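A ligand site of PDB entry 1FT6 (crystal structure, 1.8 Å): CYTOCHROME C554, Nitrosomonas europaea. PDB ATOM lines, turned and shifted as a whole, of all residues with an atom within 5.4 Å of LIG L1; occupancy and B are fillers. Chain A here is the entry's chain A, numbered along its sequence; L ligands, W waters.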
ATOM      1  N   GLY A   7     -17.106 -23.121 -13.303  1.00  0.00           N
ATOM      2  CA  GLY A   7     -16.295 -24.223 -13.777  1.00  0.00           C
ATOM      3  C   GLY A   7     -16.366 -24.320 -15.296  1.00  0.00           C
ATOM      4  O   GLY A   7     -17.094 -23.604 -15.933  1.00  0.00           O
ATOM      5  N   LYS A  10     -20.010 -26.153 -18.669  1.00  0.00           N
ATOM      6  CA  LYS A  10     -20.896 -25.552 -19.656  1.00  0.00           C
ATOM      7  C   LYS A  10     -20.170 -24.950 -20.835  1.00  0.00           C
ATOM      8  O   LYS A  10     -20.607 -25.095 -21.972  1.00  0.00           O
ATOM      9  CB  LYS A  10     -21.763 -24.479 -19.000  1.00  0.00           C
ATOM     10  CG  LYS A  10     -22.544 -25.003 -17.817  1.00  0.00           C
ATOM     11  CD  LYS A  10     -23.519 -26.046 -18.239  1.00  0.00           C
ATOM     12  CE  LYS A  10     -24.678 -26.114 -17.232  1.00  0.00           C
ATOM     13  NZ  LYS A  10     -25.615 -27.212 -17.577  1.00  0.00           N
ATOM     14  N   CYS A  11     -19.055 -24.256 -20.591  1.00  0.00           N
ATOM     15  CA  CYS A  11     -18.321 -23.665 -21.693  1.00  0.00           C
ATOM     16  C   CYS A  11     -17.846 -24.745 -22.618  1.00  0.00           C
ATOM     17  O   CYS A  11     -17.935 -24.636 -23.844  1.00  0.00           O
ATOM     18  CB  CYS A  11     -17.052 -22.921 -21.214  1.00  0.00           C
ATOM     19  SG  CYS A  11     -17.286 -21.906 -19.736  1.00  0.00           S
ATOM     20  N   SER A  13     -19.018 -27.714 -23.128  1.00  0.00           N
ATOM     21  CA  SER A  13     -20.075 -28.423 -23.831  1.00  0.00           C
ATOM     22  C   SER A  13     -20.487 -27.726 -25.123  1.00  0.00           C
ATOM     23  O   SER A  13     -20.820 -28.406 -26.086  1.00  0.00           O
ATOM     24  CB  SER A  13     -21.314 -28.608 -22.933  1.00  0.00           C
ATOM     25  OG  SER A  13     -21.994 -27.378 -22.692  1.00  0.00           O
ATOM     26  N   CYS A  14     -20.507 -26.398 -25.146  1.00  0.00           N
ATOM     27  CA  CYS A  14     -20.874 -25.638 -26.350  1.00  0.00           C
ATOM     28  C   CYS A  14     -19.675 -25.320 -27.216  1.00  0.00           C
ATOM     29  O   CYS A  14     -19.816 -25.116 -28.421  1.00  0.00           O
ATOM     30  CB  CYS A  14     -21.546 -24.302 -26.002  1.00  0.00           C
ATOM     31  SG  CYS A  14     -23.281 -24.456 -25.402  1.00  0.00           S
ATOM     32  N   HIS A  15     -18.491 -25.252 -26.624  1.00  0.00           N
ATOM     33  CA  HIS A  15     -17.293 -24.911 -27.364  1.00  0.00           C
ATOM     34  C   HIS A  15     -16.280 -26.039 -27.308  1.00  0.00           C
ATOM     35  O   HIS A  15     -15.184 -25.862 -26.772  1.00  0.00           O
ATOM     36  CB  HIS A  15     -16.667 -23.665 -26.775  1.00  0.00           C
ATOM     37  CG  HIS A  15     -17.550 -22.467 -26.787  1.00  0.00           C
ATOM     38  ND1 HIS A  15     -17.907 -21.760 -27.914  1.00  0.00           N
ATOM     39  CD2 HIS A  15     -18.099 -21.791 -25.746  1.00  0.00           C
ATOM     40  CE1 HIS A  15     -18.626 -20.709 -27.519  1.00  0.00           C
ATOM     41  NE2 HIS A  15     -18.782 -20.679 -26.193  1.00  0.00           N
ATOM     42  N   CYS A  88     -11.389 -21.995 -18.520  1.00  0.00           N
ATOM     43  CA  CYS A  88     -12.061 -20.950 -19.305  1.00  0.00           C
ATOM     44  C   CYS A  88     -12.364 -19.633 -18.626  1.00  0.00           C
ATOM     45  O   CYS A  88     -12.038 -18.582 -19.168  1.00  0.00           O
ATOM     46  CB  CYS A  88     -13.372 -21.550 -19.905  1.00  0.00           C
ATOM     47  SG  CYS A  88     -13.257 -23.294 -20.341  1.00  0.00           S
ATOM     48  N   GLU A  89     -12.937 -19.679 -17.414  1.00  0.00           N
ATOM     49  CA  GLU A  89     -13.294 -18.466 -16.679  1.00  0.00           C
ATOM     50  C   GLU A  89     -12.087 -17.715 -16.120  1.00  0.00           C
ATOM     51  O   GLU A  89     -12.203 -16.540 -15.835  1.00  0.00           O
ATOM     52  CB  GLU A  89     -14.280 -18.785 -15.551  1.00  0.00           C
ATOM     53  CG  GLU A  89     -15.634 -19.407 -16.026  1.00  0.00           C
ATOM     54  CD  GLU A  89     -16.387 -20.104 -14.874  1.00  0.00           C
ATOM     55  OE1 GLU A  89     -15.809 -21.057 -14.305  1.00  0.00           O
ATOM     56  OE2 GLU A  89     -17.522 -19.717 -14.533  1.00  0.00           O
ATOM     57  N   HIS A  92     -11.673 -15.671 -19.581  1.00  0.00           N
ATOM     58  CA  HIS A  92     -12.892 -15.034 -20.096  1.00  0.00           C
ATOM     59  C   HIS A  92     -13.765 -14.407 -18.995  1.00  0.00           C
ATOM     60  O   HIS A  92     -14.687 -13.651 -19.304  1.00  0.00           O
ATOM     61  CB  HIS A  92     -13.685 -16.092 -20.858  1.00  0.00           C
ATOM     62  CG  HIS A  92     -13.001 -16.544 -22.097  1.00  0.00           C
ATOM     63  ND1 HIS A  92     -12.786 -15.711 -23.168  1.00  0.00           N
ATOM     64  CD2 HIS A  92     -12.348 -17.704 -22.378  1.00  0.00           C
ATOM     65  CE1 HIS A  92     -12.035 -16.342 -24.055  1.00  0.00           C
ATOM     66  NE2 HIS A  92     -11.728 -17.553 -23.654  1.00  0.00           N
ATOM     67  N   GLY A  93     -13.451 -14.721 -17.735  1.00  0.00           N
ATOM     68  CA  GLY A  93     -14.186 -14.198 -16.599  1.00  0.00           C
ATOM     69  C   GLY A  93     -15.231 -15.176 -16.098  1.00  0.00           C
ATOM     70  O   GLY A  93     -15.565 -16.094 -16.816  1.00  0.00           O
ATOM     71  N   GLY A  95     -18.452 -17.089 -15.580  1.00  0.00           N
ATOM     72  CA  GLY A  95     -19.518 -17.222 -16.547  1.00  0.00           C
ATOM     73  C   GLY A  95     -20.944 -17.376 -16.149  1.00  0.00           C
ATOM     74  O   GLY A  95     -21.790 -17.412 -17.054  1.00  0.00           O
ATOM     75  N   PHE A  98     -23.069 -14.498 -18.016  1.00  0.00           N
ATOM     76  CA  PHE A  98     -22.988 -14.351 -19.453  1.00  0.00           C
ATOM     77  C   PHE A  98     -23.205 -15.651 -20.231  1.00  0.00           C
ATOM     78  O   PHE A  98     -23.627 -15.603 -21.378  1.00  0.00           O
ATOM     79  CB  PHE A  98     -21.677 -13.658 -19.896  1.00  0.00           C
ATOM     80  CG  PHE A  98     -20.416 -14.520 -19.776  1.00  0.00           C
ATOM     81  CD1 PHE A  98     -20.228 -15.641 -20.590  1.00  0.00           C
ATOM     82  CD2 PHE A  98     -19.371 -14.116 -18.922  1.00  0.00           C
ATOM     83  CE1 PHE A  98     -19.025 -16.370 -20.580  1.00  0.00           C
ATOM     84  CE2 PHE A  98     -18.150 -14.818 -18.894  1.00  0.00           C
ATOM     85  CZ  PHE A  98     -17.973 -15.965 -19.733  1.00  0.00           C
ATOM     86  N   ARG A  99     -23.007 -16.803 -19.643  1.00  0.00           N
ATOM     87  CA  ARG A  99     -23.202 -17.967 -20.467  1.00  0.00           C
ATOM     88  C   ARG A  99     -24.644 -18.135 -20.921  1.00  0.00           C
ATOM     89  O   ARG A  99     -24.898 -18.798 -21.932  1.00  0.00           O
ATOM     90  CB  ARG A  99     -22.701 -19.224 -19.768  1.00  0.00           C
ATOM     91  CG  ARG A  99     -23.549 -19.703 -18.635  1.00  0.00           C
ATOM     92  CD  ARG A  99     -23.090 -21.084 -18.174  1.00  0.00           C
ATOM     93  NE  ARG A  99     -23.687 -21.462 -16.894  1.00  0.00           N
ATOM     94  CZ  ARG A  99     -24.900 -21.981 -16.770  1.00  0.00           C
ATOM     95  NH1 ARG A  99     -25.642 -22.189 -17.842  1.00  0.00           N
ATOM     96  NH2 ARG A  99     -25.372 -22.313 -15.563  1.00  0.00           N
ATOM     97  N   HIS A 102     -25.013 -16.338 -24.031  1.00  0.00           N
ATOM     98  CA  HIS A 102     -24.422 -17.057 -25.171  1.00  0.00           C
ATOM     99  C   HIS A 102     -25.478 -18.030 -25.726  1.00  0.00           C
ATOM    100  O   HIS A 102     -25.615 -18.199 -26.962  1.00  0.00           O
ATOM    101  CB  HIS A 102     -23.188 -17.844 -24.770  1.00  0.00           C
ATOM    102  CG  HIS A 102     -21.989 -16.979 -24.510  1.00  0.00           C
ATOM    103  ND1 HIS A 102     -20.696 -17.469 -24.617  1.00  0.00           N
ATOM    104  CD2 HIS A 102     -21.946 -15.683 -24.137  1.00  0.00           C
ATOM    105  CE1 HIS A 102     -19.925 -16.448 -24.296  1.00  0.00           C
ATOM    106  NE2 HIS A 102     -20.621 -15.356 -24.003  1.00  0.00           N
ATOM    107  N   ARG A 103     -26.215 -18.665 -24.823  1.00  0.00           N
ATOM    108  CA  ARG A 103     -27.276 -19.583 -25.255  1.00  0.00           C
ATOM    109  C   ARG A 103     -28.381 -18.835 -26.006  1.00  0.00           C
ATOM    110  O   ARG A 103     -28.682 -19.147 -27.168  1.00  0.00           O
ATOM    111  CB  ARG A 103     -27.924 -20.307 -24.073  1.00  0.00           C
ATOM    112  CG  ARG A 103     -28.855 -21.457 -24.496  1.00  0.00           C
ATOM    113  CD  ARG A 103     -29.672 -22.035 -23.334  1.00  0.00           C
ATOM    114  NE  ARG A 103     -31.115 -21.910 -23.548  1.00  0.00           N
ATOM    115  CZ  ARG A 103     -31.905 -22.880 -23.997  1.00  0.00           C
ATOM    116  NH1 ARG A 103     -31.406 -24.070 -24.288  1.00  0.00           N
ATOM    117  NH2 ARG A 103     -33.215 -22.664 -24.177  1.00  0.00           N
ATOM    118  N   GLY A 106     -27.221 -17.198 -29.322  1.00  0.00           N
ATOM    119  CA  GLY A 106     -26.909 -18.195 -30.334  1.00  0.00           C
ATOM    120  C   GLY A 106     -28.196 -18.707 -30.937  1.00  0.00           C
ATOM    121  O   GLY A 106     -28.286 -18.969 -32.130  1.00  0.00           O
ATOM    122  N   ARG A 118     -21.501  -7.027 -28.014  1.00  0.00           N
ATOM    123  CA  ARG A 118     -20.587  -7.527 -26.970  1.00  0.00           C
ATOM    124  C   ARG A 118     -20.832  -6.743 -25.660  1.00  0.00           C
ATOM    125  O   ARG A 118     -20.602  -7.257 -24.569  1.00  0.00           O
ATOM    126  CB  ARG A 118     -19.138  -7.351 -27.400  1.00  0.00           C
ATOM    127  CG  ARG A 118     -18.627  -8.516 -28.181  1.00  0.00           C
ATOM    128  CD  ARG A 118     -17.191  -8.321 -28.665  1.00  0.00           C
ATOM    129  NE  ARG A 118     -16.969  -9.431 -29.585  1.00  0.00           N
ATOM    130  CZ  ARG A 118     -16.993  -9.298 -30.902  1.00  0.00           C
ATOM    131  NH1 ARG A 118     -17.228  -8.106 -31.441  1.00  0.00           N
ATOM    132  NH2 ARG A 118     -16.861 -10.357 -31.671  1.00  0.00           N
ATOM    133  N   LEU A 121     -22.590  -8.532 -23.066  1.00  0.00           N
ATOM    134  CA  LEU A 121     -21.846  -9.601 -22.393  1.00  0.00           C
ATOM    135  C   LEU A 121     -20.896  -9.016 -21.363  1.00  0.00           C
ATOM    136  O   LEU A 121     -20.717  -9.592 -20.295  1.00  0.00           O
ATOM    137  CB  LEU A 121     -21.055 -10.464 -23.398  1.00  0.00           C
ATOM    138  CG  LEU A 121     -21.868 -11.269 -24.438  1.00  0.00           C
ATOM    139  CD1 LEU A 121     -20.871 -11.961 -25.392  1.00  0.00           C
ATOM    140  CD2 LEU A 121     -22.755 -12.330 -23.771  1.00  0.00           C
ATOM    141  N   GLN A 126     -18.291 -10.582 -18.811  1.00  0.00           N
ATOM    142  CA  GLN A 126     -17.314 -11.216 -19.728  1.00  0.00           C
ATOM    143  C   GLN A 126     -16.116 -10.323 -19.971  1.00  0.00           C
ATOM    144  O   GLN A 126     -16.214  -9.085 -20.084  1.00  0.00           O
ATOM    145  CB  GLN A 126     -17.955 -11.590 -21.096  1.00  0.00           C
ATOM    146  CG  GLN A 126     -16.975 -12.373 -22.041  1.00  0.00           C
ATOM    147  CD  GLN A 126     -17.700 -13.283 -23.054  1.00  0.00           C
ATOM    148  OE1 GLN A 126     -18.951 -13.324 -23.042  1.00  0.00           O
ATOM    149  NE2 GLN A 126     -17.033 -13.964 -23.868  1.00  0.00           N
ATOM    150  N   PHE A 128     -13.176  -9.069 -22.320  1.00  0.00           N
ATOM    151  CA  PHE A 128     -12.682  -8.997 -23.721  1.00  0.00           C
ATOM    152  C   PHE A 128     -11.319  -8.298 -23.807  1.00  0.00           C
ATOM    153  O   PHE A 128     -10.884  -7.945 -24.911  1.00  0.00           O
ATOM    154  CB  PHE A 128     -13.669  -8.247 -24.594  1.00  0.00           C
ATOM    155  CG  PHE A 128     -15.017  -8.910 -24.632  1.00  0.00           C
ATOM    156  CD1 PHE A 128     -15.282  -9.931 -25.549  1.00  0.00           C
ATOM    157  CD2 PHE A 128     -15.999  -8.563 -23.697  1.00  0.00           C
ATOM    158  CE1 PHE A 128     -16.517 -10.605 -25.533  1.00  0.00           C
ATOM    159  CE2 PHE A 128     -17.231  -9.219 -23.664  1.00  0.00           C
ATOM    160  CZ  PHE A 128     -17.498 -10.250 -24.583  1.00  0.00           C
ATOM    161  N   LYS A 183     -12.930 -20.343 -36.197  1.00  0.00           N
ATOM    162  CA  LYS A 183     -13.805 -19.324 -36.762  1.00  0.00           C
ATOM    163  C   LYS A 183     -15.162 -19.206 -36.042  1.00  0.00           C
ATOM    164  O   LYS A 183     -15.766 -20.220 -35.671  1.00  0.00           O
ATOM    165  CB  LYS A 183     -14.057 -19.627 -38.251  1.00  0.00           C
ATOM    166  CG  LYS A 183     -14.500 -18.407 -39.035  1.00  0.00           C
ATOM    167  CD  LYS A 183     -13.334 -17.461 -39.334  1.00  0.00           C
ATOM    168  CE  LYS A 183     -12.253 -18.138 -40.180  1.00  0.00           C
ATOM    169  NZ  LYS A 183     -11.385 -17.156 -40.922  1.00  0.00           N
ATOM    170  N   LEU A 184     -15.615 -17.968 -35.845  1.00  0.00           N
ATOM    171  CA  LEU A 184     -16.912 -17.680 -35.230  1.00  0.00           C
ATOM    172  C   LEU A 184     -17.900 -17.371 -36.364  1.00  0.00           C
ATOM    173  O   LEU A 184     -17.472 -16.901 -37.430  1.00  0.00           O
ATOM    174  CB  LEU A 184     -16.829 -16.461 -34.333  1.00  0.00           C
ATOM    175  CG  LEU A 184     -15.994 -16.709 -33.054  1.00  0.00           C
ATOM    176  CD1 LEU A 184     -15.547 -15.358 -32.484  1.00  0.00           C
ATOM    177  CD2 LEU A 184     -16.821 -17.469 -32.046  1.00  0.00           C
ATOM    178  N   GLU A 185     -19.187 -17.629 -36.153  1.00  0.00           N
ATOM    179  CA  GLU A 185     -20.203 -17.335 -37.160  1.00  0.00           C
ATOM    180  C   GLU A 185     -20.494 -15.852 -37.109  1.00  0.00           C
ATOM    181  O   GLU A 185     -20.970 -15.272 -38.088  1.00  0.00           O
ATOM    182  CB  GLU A 185     -21.505 -18.095 -36.905  1.00  0.00           C
ATOM    183  CG  GLU A 185     -21.467 -19.587 -37.106  1.00  0.00           C
ATOM    184  CD  GLU A 185     -20.769 -19.972 -38.400  1.00  0.00           C
ATOM    185  OE1 GLU A 185     -20.943 -19.253 -39.405  1.00  0.00           O
ATOM    186  OE2 GLU A 185     -20.028 -20.989 -38.398  1.00  0.00           O
ATOM    187  N   GLY A 186     -20.248 -15.216 -35.966  1.00  0.00           N
ATOM    188  CA  GLY A 186     -20.481 -13.787 -35.873  1.00  0.00           C
ATOM    189  C   GLY A 186     -21.693 -13.373 -35.063  1.00  0.00           C
ATOM    190  O   GLY A 186     -22.262 -12.297 -35.287  1.00  0.00           O
ATOM    191  N   VAL A 187     -22.098 -14.218 -34.106  1.00  0.00           N
ATOM    192  CA  VAL A 187     -23.263 -13.943 -33.294  1.00  0.00           C
ATOM    193  C   VAL A 187     -23.149 -12.603 -32.573  1.00  0.00           C
ATOM    194  O   VAL A 187     -24.104 -11.843 -32.509  1.00  0.00           O
ATOM    195  CB  VAL A 187     -23.476 -15.045 -32.267  1.00  0.00           C
ATOM    196  CG1 VAL A 187     -24.554 -14.627 -31.243  1.00  0.00           C
ATOM    197  CG2 VAL A 187     -23.904 -16.339 -32.972  1.00  0.00           C
ATOM    198  N   PHE A 188     -21.964 -12.337 -32.018  1.00  0.00           N
ATOM    199  CA  PHE A 188     -21.727 -11.105 -31.277  1.00  0.00           C
ATOM    200  C   PHE A 188     -20.973 -10.051 -32.072  1.00  0.00           C
ATOM    201  O   PHE A 188     -20.159 -10.388 -32.933  1.00  0.00           O
ATOM    202  CB  PHE A 188     -20.971 -11.428 -29.979  1.00  0.00           C
ATOM    203  CG  PHE A 188     -21.729 -12.359 -29.046  1.00  0.00           C
ATOM    204  CD1 PHE A 188     -21.343 -13.698 -28.892  1.00  0.00           C
ATOM    205  CD2 PHE A 188     -22.853 -11.900 -28.344  1.00  0.00           C
ATOM    206  CE1 PHE A 188     -22.073 -14.556 -28.070  1.00  0.00           C
ATOM    207  CE2 PHE A 188     -23.575 -12.750 -27.514  1.00  0.00           C
ATOM    208  CZ  PHE A 188     -23.197 -14.088 -27.367  1.00  0.00           C
ATOM    209  N   HIS A 197      -8.726  -9.732 -31.795  1.00  0.00           N
ATOM    210  CA  HIS A 197      -9.843 -10.594 -32.213  1.00  0.00           C
ATOM    211  C   HIS A 197      -9.899 -10.805 -33.733  1.00  0.00           C
ATOM    212  O   HIS A 197      -9.997 -11.937 -34.211  1.00  0.00           O
ATOM    213  CB  HIS A 197     -11.190  -9.972 -31.765  1.00  0.00           C
ATOM    214  CG  HIS A 197     -12.397 -10.739 -32.211  1.00  0.00           C
ATOM    215  ND1 HIS A 197     -12.957 -11.768 -31.479  1.00  0.00           N
ATOM    216  CD2 HIS A 197     -13.146 -10.633 -33.340  1.00  0.00           C
ATOM    217  CE1 HIS A 197     -13.987 -12.262 -32.138  1.00  0.00           C
ATOM    218  NE2 HIS A 197     -14.129 -11.599 -33.280  1.00  0.00           N
HETATM  219 FE1  LIG L   1     -19.750 -19.096 -25.458  1.00  0.00          FE
HETATM  220  C1  LIG L   1     -19.258 -17.143 -28.189  1.00  0.00           C
HETATM  221  C2  LIG L   1     -16.803 -18.177 -24.198  1.00  0.00           C
HETATM  222  C3  LIG L   1     -20.425 -20.877 -22.565  1.00  0.00           C
HETATM  223  C4  LIG L   1     -22.475 -20.487 -26.956  1.00  0.00           C
HETATM  224  N1  LIG L   1     -18.318 -17.945 -26.081  1.00  0.00           N
HETATM  225  C5  LIG L   1     -18.275 -17.175 -27.209  1.00  0.00           C
HETATM  226  C6  LIG L   1     -17.081 -16.409 -27.263  1.00  0.00           C
HETATM  227  C7  LIG L   1     -16.346 -16.744 -26.152  1.00  0.00           C
HETATM  228  C8  LIG L   1     -17.143 -17.670 -25.439  1.00  0.00           C
HETATM  229  C9  LIG L   1     -14.942 -16.173 -25.713  1.00  0.00           C
HETATM  230  C10 LIG L   1     -16.715 -15.437 -28.366  1.00  0.00           C
HETATM  231  C11 LIG L   1     -17.235 -14.014 -28.050  1.00  0.00           C
HETATM  232  C12 LIG L   1     -16.846 -12.926 -29.058  1.00  0.00           C
HETATM  233  O1  LIG L   1     -17.313 -13.011 -30.237  1.00  0.00           O
HETATM  234  O2  LIG L   1     -16.130 -11.955 -28.694  1.00  0.00           O
HETATM  235  N2  LIG L   1     -18.818 -19.470 -23.726  1.00  0.00           N
HETATM  236  C13 LIG L   1     -17.564 -18.998 -23.392  1.00  0.00           C
HETATM  237  C14 LIG L   1     -17.171 -19.383 -22.057  1.00  0.00           C
HETATM  238  C15 LIG L   1     -18.218 -20.089 -21.539  1.00  0.00           C
HETATM  239  C16 LIG L   1     -19.250 -20.148 -22.624  1.00  0.00           C
HETATM  240  C17 LIG L   1     -15.841 -19.077 -21.333  1.00  0.00           C
HETATM  241  C18 LIG L   1     -18.355 -20.754 -20.138  1.00  0.00           C
HETATM  242  C19 LIG L   1     -18.572 -19.761 -19.035  1.00  0.00           C
HETATM  243  N3  LIG L   1     -21.140 -20.358 -24.879  1.00  0.00           N
HETATM  244  C20 LIG L   1     -21.268 -21.032 -23.637  1.00  0.00           C
HETATM  245  C21 LIG L   1     -22.351 -21.988 -23.632  1.00  0.00           C
HETATM  246  C22 LIG L   1     -22.849 -21.954 -24.908  1.00  0.00           C
HETATM  247  C23 LIG L   1     -22.152 -20.920 -25.648  1.00  0.00           C
HETATM  248  C24 LIG L   1     -22.795 -22.906 -22.478  1.00  0.00           C
HETATM  249  C25 LIG L   1     -23.919 -22.924 -25.477  1.00  0.00           C
HETATM  250  C26 LIG L   1     -25.304 -22.959 -24.870  1.00  0.00           C
HETATM  251  N4  LIG L   1     -20.714 -18.809 -27.195  1.00  0.00           N
HETATM  252  C27 LIG L   1     -21.832 -19.484 -27.650  1.00  0.00           C
HETATM  253  C28 LIG L   1     -22.247 -18.985 -28.977  1.00  0.00           C
HETATM  254  C29 LIG L   1     -21.326 -18.010 -29.277  1.00  0.00           C
HETATM  255  C30 LIG L   1     -20.391 -17.931 -28.175  1.00  0.00           C
HETATM  256  C31 LIG L   1     -23.443 -19.513 -29.840  1.00  0.00           C
HETATM  257  C32 LIG L   1     -21.160 -17.354 -30.637  1.00  0.00           C
HETATM  258  C33 LIG L   1     -20.245 -18.141 -31.575  1.00  0.00           C
HETATM  259  C34 LIG L   1     -20.121 -17.588 -32.963  1.00  0.00           C
HETATM  260  O3  LIG L   1     -19.959 -18.427 -33.880  1.00  0.00           O
HETATM  261  O4  LIG L   1     -20.155 -16.355 -33.098  1.00  0.00           O
HETATM  262 FE1  LG2 L   2     -10.693 -18.910 -24.765  1.00  0.00          FE
HETATM  263  C1  LG2 L   2     -11.169 -16.963 -27.475  1.00  0.00           C
HETATM  264  C2  LG2 L   2     -13.584 -20.657 -25.526  1.00  0.00           C
HETATM  265  C3  LG2 L   2     -10.079 -21.051 -22.177  1.00  0.00           C
HETATM  266  C4  LG2 L   2      -8.047 -16.996 -23.822  1.00  0.00           C
HETATM  267  N1  LG2 L   2     -12.085 -18.813 -26.225  1.00  0.00           N
HETATM  268  C5  LG2 L   2     -12.115 -17.955 -27.255  1.00  0.00           C
HETATM  269  C6  LG2 L   2     -13.288 -18.172 -28.104  1.00  0.00           C
HETATM  270  C7  LG2 L   2     -14.010 -19.212 -27.514  1.00  0.00           C
HETATM  271  C8  LG2 L   2     -13.238 -19.609 -26.355  1.00  0.00           C
HETATM  272  C9  LG2 L   2     -15.326 -19.891 -27.911  1.00  0.00           C
HETATM  273  C10 LG2 L   2     -13.627 -17.340 -29.406  1.00  0.00           C
HETATM  274  C11 LG2 L   2     -13.283 -18.133 -30.675  1.00  0.00           C
HETATM  275  C12 LG2 L   2     -11.820 -18.627 -30.756  1.00  0.00           C
HETATM  276  O1  LG2 L   2     -10.946 -17.769 -30.673  1.00  0.00           O
HETATM  277  O2  LG2 L   2     -11.599 -19.858 -30.872  1.00  0.00           O
HETATM  278  N2  LG2 L   2     -11.627 -20.457 -24.002  1.00  0.00           N
HETATM  279  C13 LG2 L   2     -12.831 -21.088 -24.400  1.00  0.00           C
HETATM  280  C14 LG2 L   2     -13.167 -22.226 -23.592  1.00  0.00           C
HETATM  281  C15 LG2 L   2     -12.190 -22.354 -22.647  1.00  0.00           C
HETATM  282  C16 LG2 L   2     -11.229 -21.283 -22.935  1.00  0.00           C
HETATM  283  C17 LG2 L   2     -14.384 -23.194 -23.745  1.00  0.00           C
HETATM  284  C18 LG2 L   2     -12.044 -23.392 -21.522  1.00  0.00           C
HETATM  285  C19 LG2 L   2     -11.825 -24.859 -21.991  1.00  0.00           C
HETATM  286  N3  LG2 L   2      -9.316 -19.014 -23.321  1.00  0.00           N
HETATM  287  C20 LG2 L   2      -9.212 -19.965 -22.347  1.00  0.00           C
HETATM  288  C21 LG2 L   2      -8.130 -19.683 -21.446  1.00  0.00           C
HETATM  289  C22 LG2 L   2      -7.615 -18.503 -21.829  1.00  0.00           C
HETATM  290  C23 LG2 L   2      -8.346 -18.113 -23.047  1.00  0.00           C
HETATM  291  C24 LG2 L   2      -7.708 -20.575 -20.217  1.00  0.00           C
HETATM  292  C25 LG2 L   2      -6.499 -17.660 -21.121  1.00  0.00           C
HETATM  293  C26 LG2 L   2      -5.183 -18.420 -20.988  1.00  0.00           C
HETATM  294  N4  LG2 L   2      -9.756 -17.405 -25.528  1.00  0.00           N
HETATM  295  C27 LG2 L   2      -8.706 -16.659 -25.012  1.00  0.00           C
HETATM  296  C28 LG2 L   2      -8.377 -15.519 -25.827  1.00  0.00           C
HETATM  297  C29 LG2 L   2      -9.255 -15.552 -26.874  1.00  0.00           C
HETATM  298  C30 LG2 L   2     -10.068 -16.681 -26.667  1.00  0.00           C
HETATM  299  C31 LG2 L   2      -7.290 -14.477 -25.506  1.00  0.00           C
HETATM  300  C32 LG2 L   2      -9.430 -14.466 -27.956  1.00  0.00           C
HETATM  301  C33 LG2 L   2     -10.504 -13.430 -27.725  1.00  0.00           C
HETATM  302  C34 LG2 L   2     -11.103 -12.861 -29.033  1.00  0.00           C
HETATM  303  O3  LG2 L   2     -12.175 -12.253 -28.947  1.00  0.00           O
HETATM  304  O4  LG2 L   2     -10.494 -13.018 -30.131  1.00  0.00           O
HETATM  305  O   HOH W   1     -13.529  -9.839 -28.514  1.00  0.00           O
HETATM  306  O   HOH W   2     -19.297 -13.851 -31.815  1.00  0.00           O
HETATM  307  O   HOH W   3     -14.116 -13.011 -26.887  1.00  0.00           O
HETATM  308  O   HOH W   4     -14.143 -13.256 -24.201  1.00  0.00           O
HETATM  309  O   HOH W   5     -19.953 -20.349 -15.899  1.00  0.00           O
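FE1 of LG2 L2 is bound by NE2 of His 92, 2.0 Å away. ND1 of His 102 binds FE1 of LIG L1, at 2.1 Å. NE2 of His 15 binds FE1 of LIG L1. An oxygen (O3) of LG2 L2 lies within hydrogen-bond range of a ring nitrogen (ND1) of His 197, at 2.7 Å. N of Val 187 is in hydrogen-bond range of O4 of LIG L1 (3.1 Å). The side-chain sulfur (SG) of Cys 88 is bonded to a carbon (C18) of LG2 L2, at 1.7 Å. The backbone NH (N) of Gly 186 sits at hydrogen-bond distance from an oxygen (O4) of LIG L1 (3.1 Å). The guanidinium group of Arg 118 is in salt-bridge range of an oxygen (O2) of LIG L1 (2.8 Å). The side-chain sulfur of Cys 14 is bonded to a carbon (C25) of LIG L1, at 1.7 Å. The side-chain sulfur of Cys 11 is covalently linked to a carbon (C18) of LIG L1. The backbone NH (N) of Glu 185 sits at hydrogen-bond distance from an oxygen (O3) of LIG L1 (2.5 Å).
A ring nitrogen (NE2) of His 102 lies within hydrogen-bond range of the side-chain amide oxygen (OE1) of Gln 126. O of Lys 10 sits at hydrogen-bond distance from OG of Ser 13, at 2.8 Å. The backbone carbonyl oxygen (O) of Leu 121 sits at hydrogen-bond distance from the backbone NH (N) of Gln 126 (3.0 Å). The backbone NH (N) of Gly 95 sits at hydrogen-bond distance from the side-chain carboxylate (OE2) of Glu 89, 3.0 Å away. The guanidinium group (NH2) of Arg 118 sits at hydrogen-bond distance from a ring nitrogen (NE2) of His 197.
O of Lys 10 touches C24 of LIG L1, at 3.1 Å. CB of Cys 88 touches C17 of LIG L1, 3.8 Å away. His 92 touches LIG L1 (CE1 to C9, 3.4 Å). Gly 95 touches LIG L1. Phe 98 touches LIG L1. CB of Arg 99 touches C3 of LIG L1, at 3.97 Å. CB of Arg 103 touches C26 of LIG L1, 3.8 Å away. CA of Gly 106 touches C31 of LIG L1, at 3.7 Å. Gln 126 touches LIG L1. Phe 128 touches LIG L1 (CE1 to O2, 3.5 Å). C of Leu 184 touches O3 of LIG L1, 3.4 Å away. CE1 of Phe 188 touches C29 of LIG L1, at 3.7 Å. CE1 of His 197 touches O1 of LIG L1 (3.9 Å). Hydrophobic or aromatic side chains that line LIG L1: His 15, His 92, Phe 98, His 102, Phe 128, Leu 184, Val 187, Phe 188 and His 197. The nearest printed residue that does not touch LIG L1 is Glu 89 (4.2 Å).
Water W2 lies within hydrogen-bond range of an oxygen (O1) of LIG L1 (2.7 Å) and the backbone NH (N) of Phe 188 (3.1 Å). Water W3 bridges O2 of LIG L1 and O3 of LG2 L2. Water W1 bridges O3 of LG2 L2 and O2 of LIG L1. Water W4 lies within hydrogen-bond range of ND1 of His 92 (3.0 Å) and NE2 of Gln 126 (3.0 Å).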
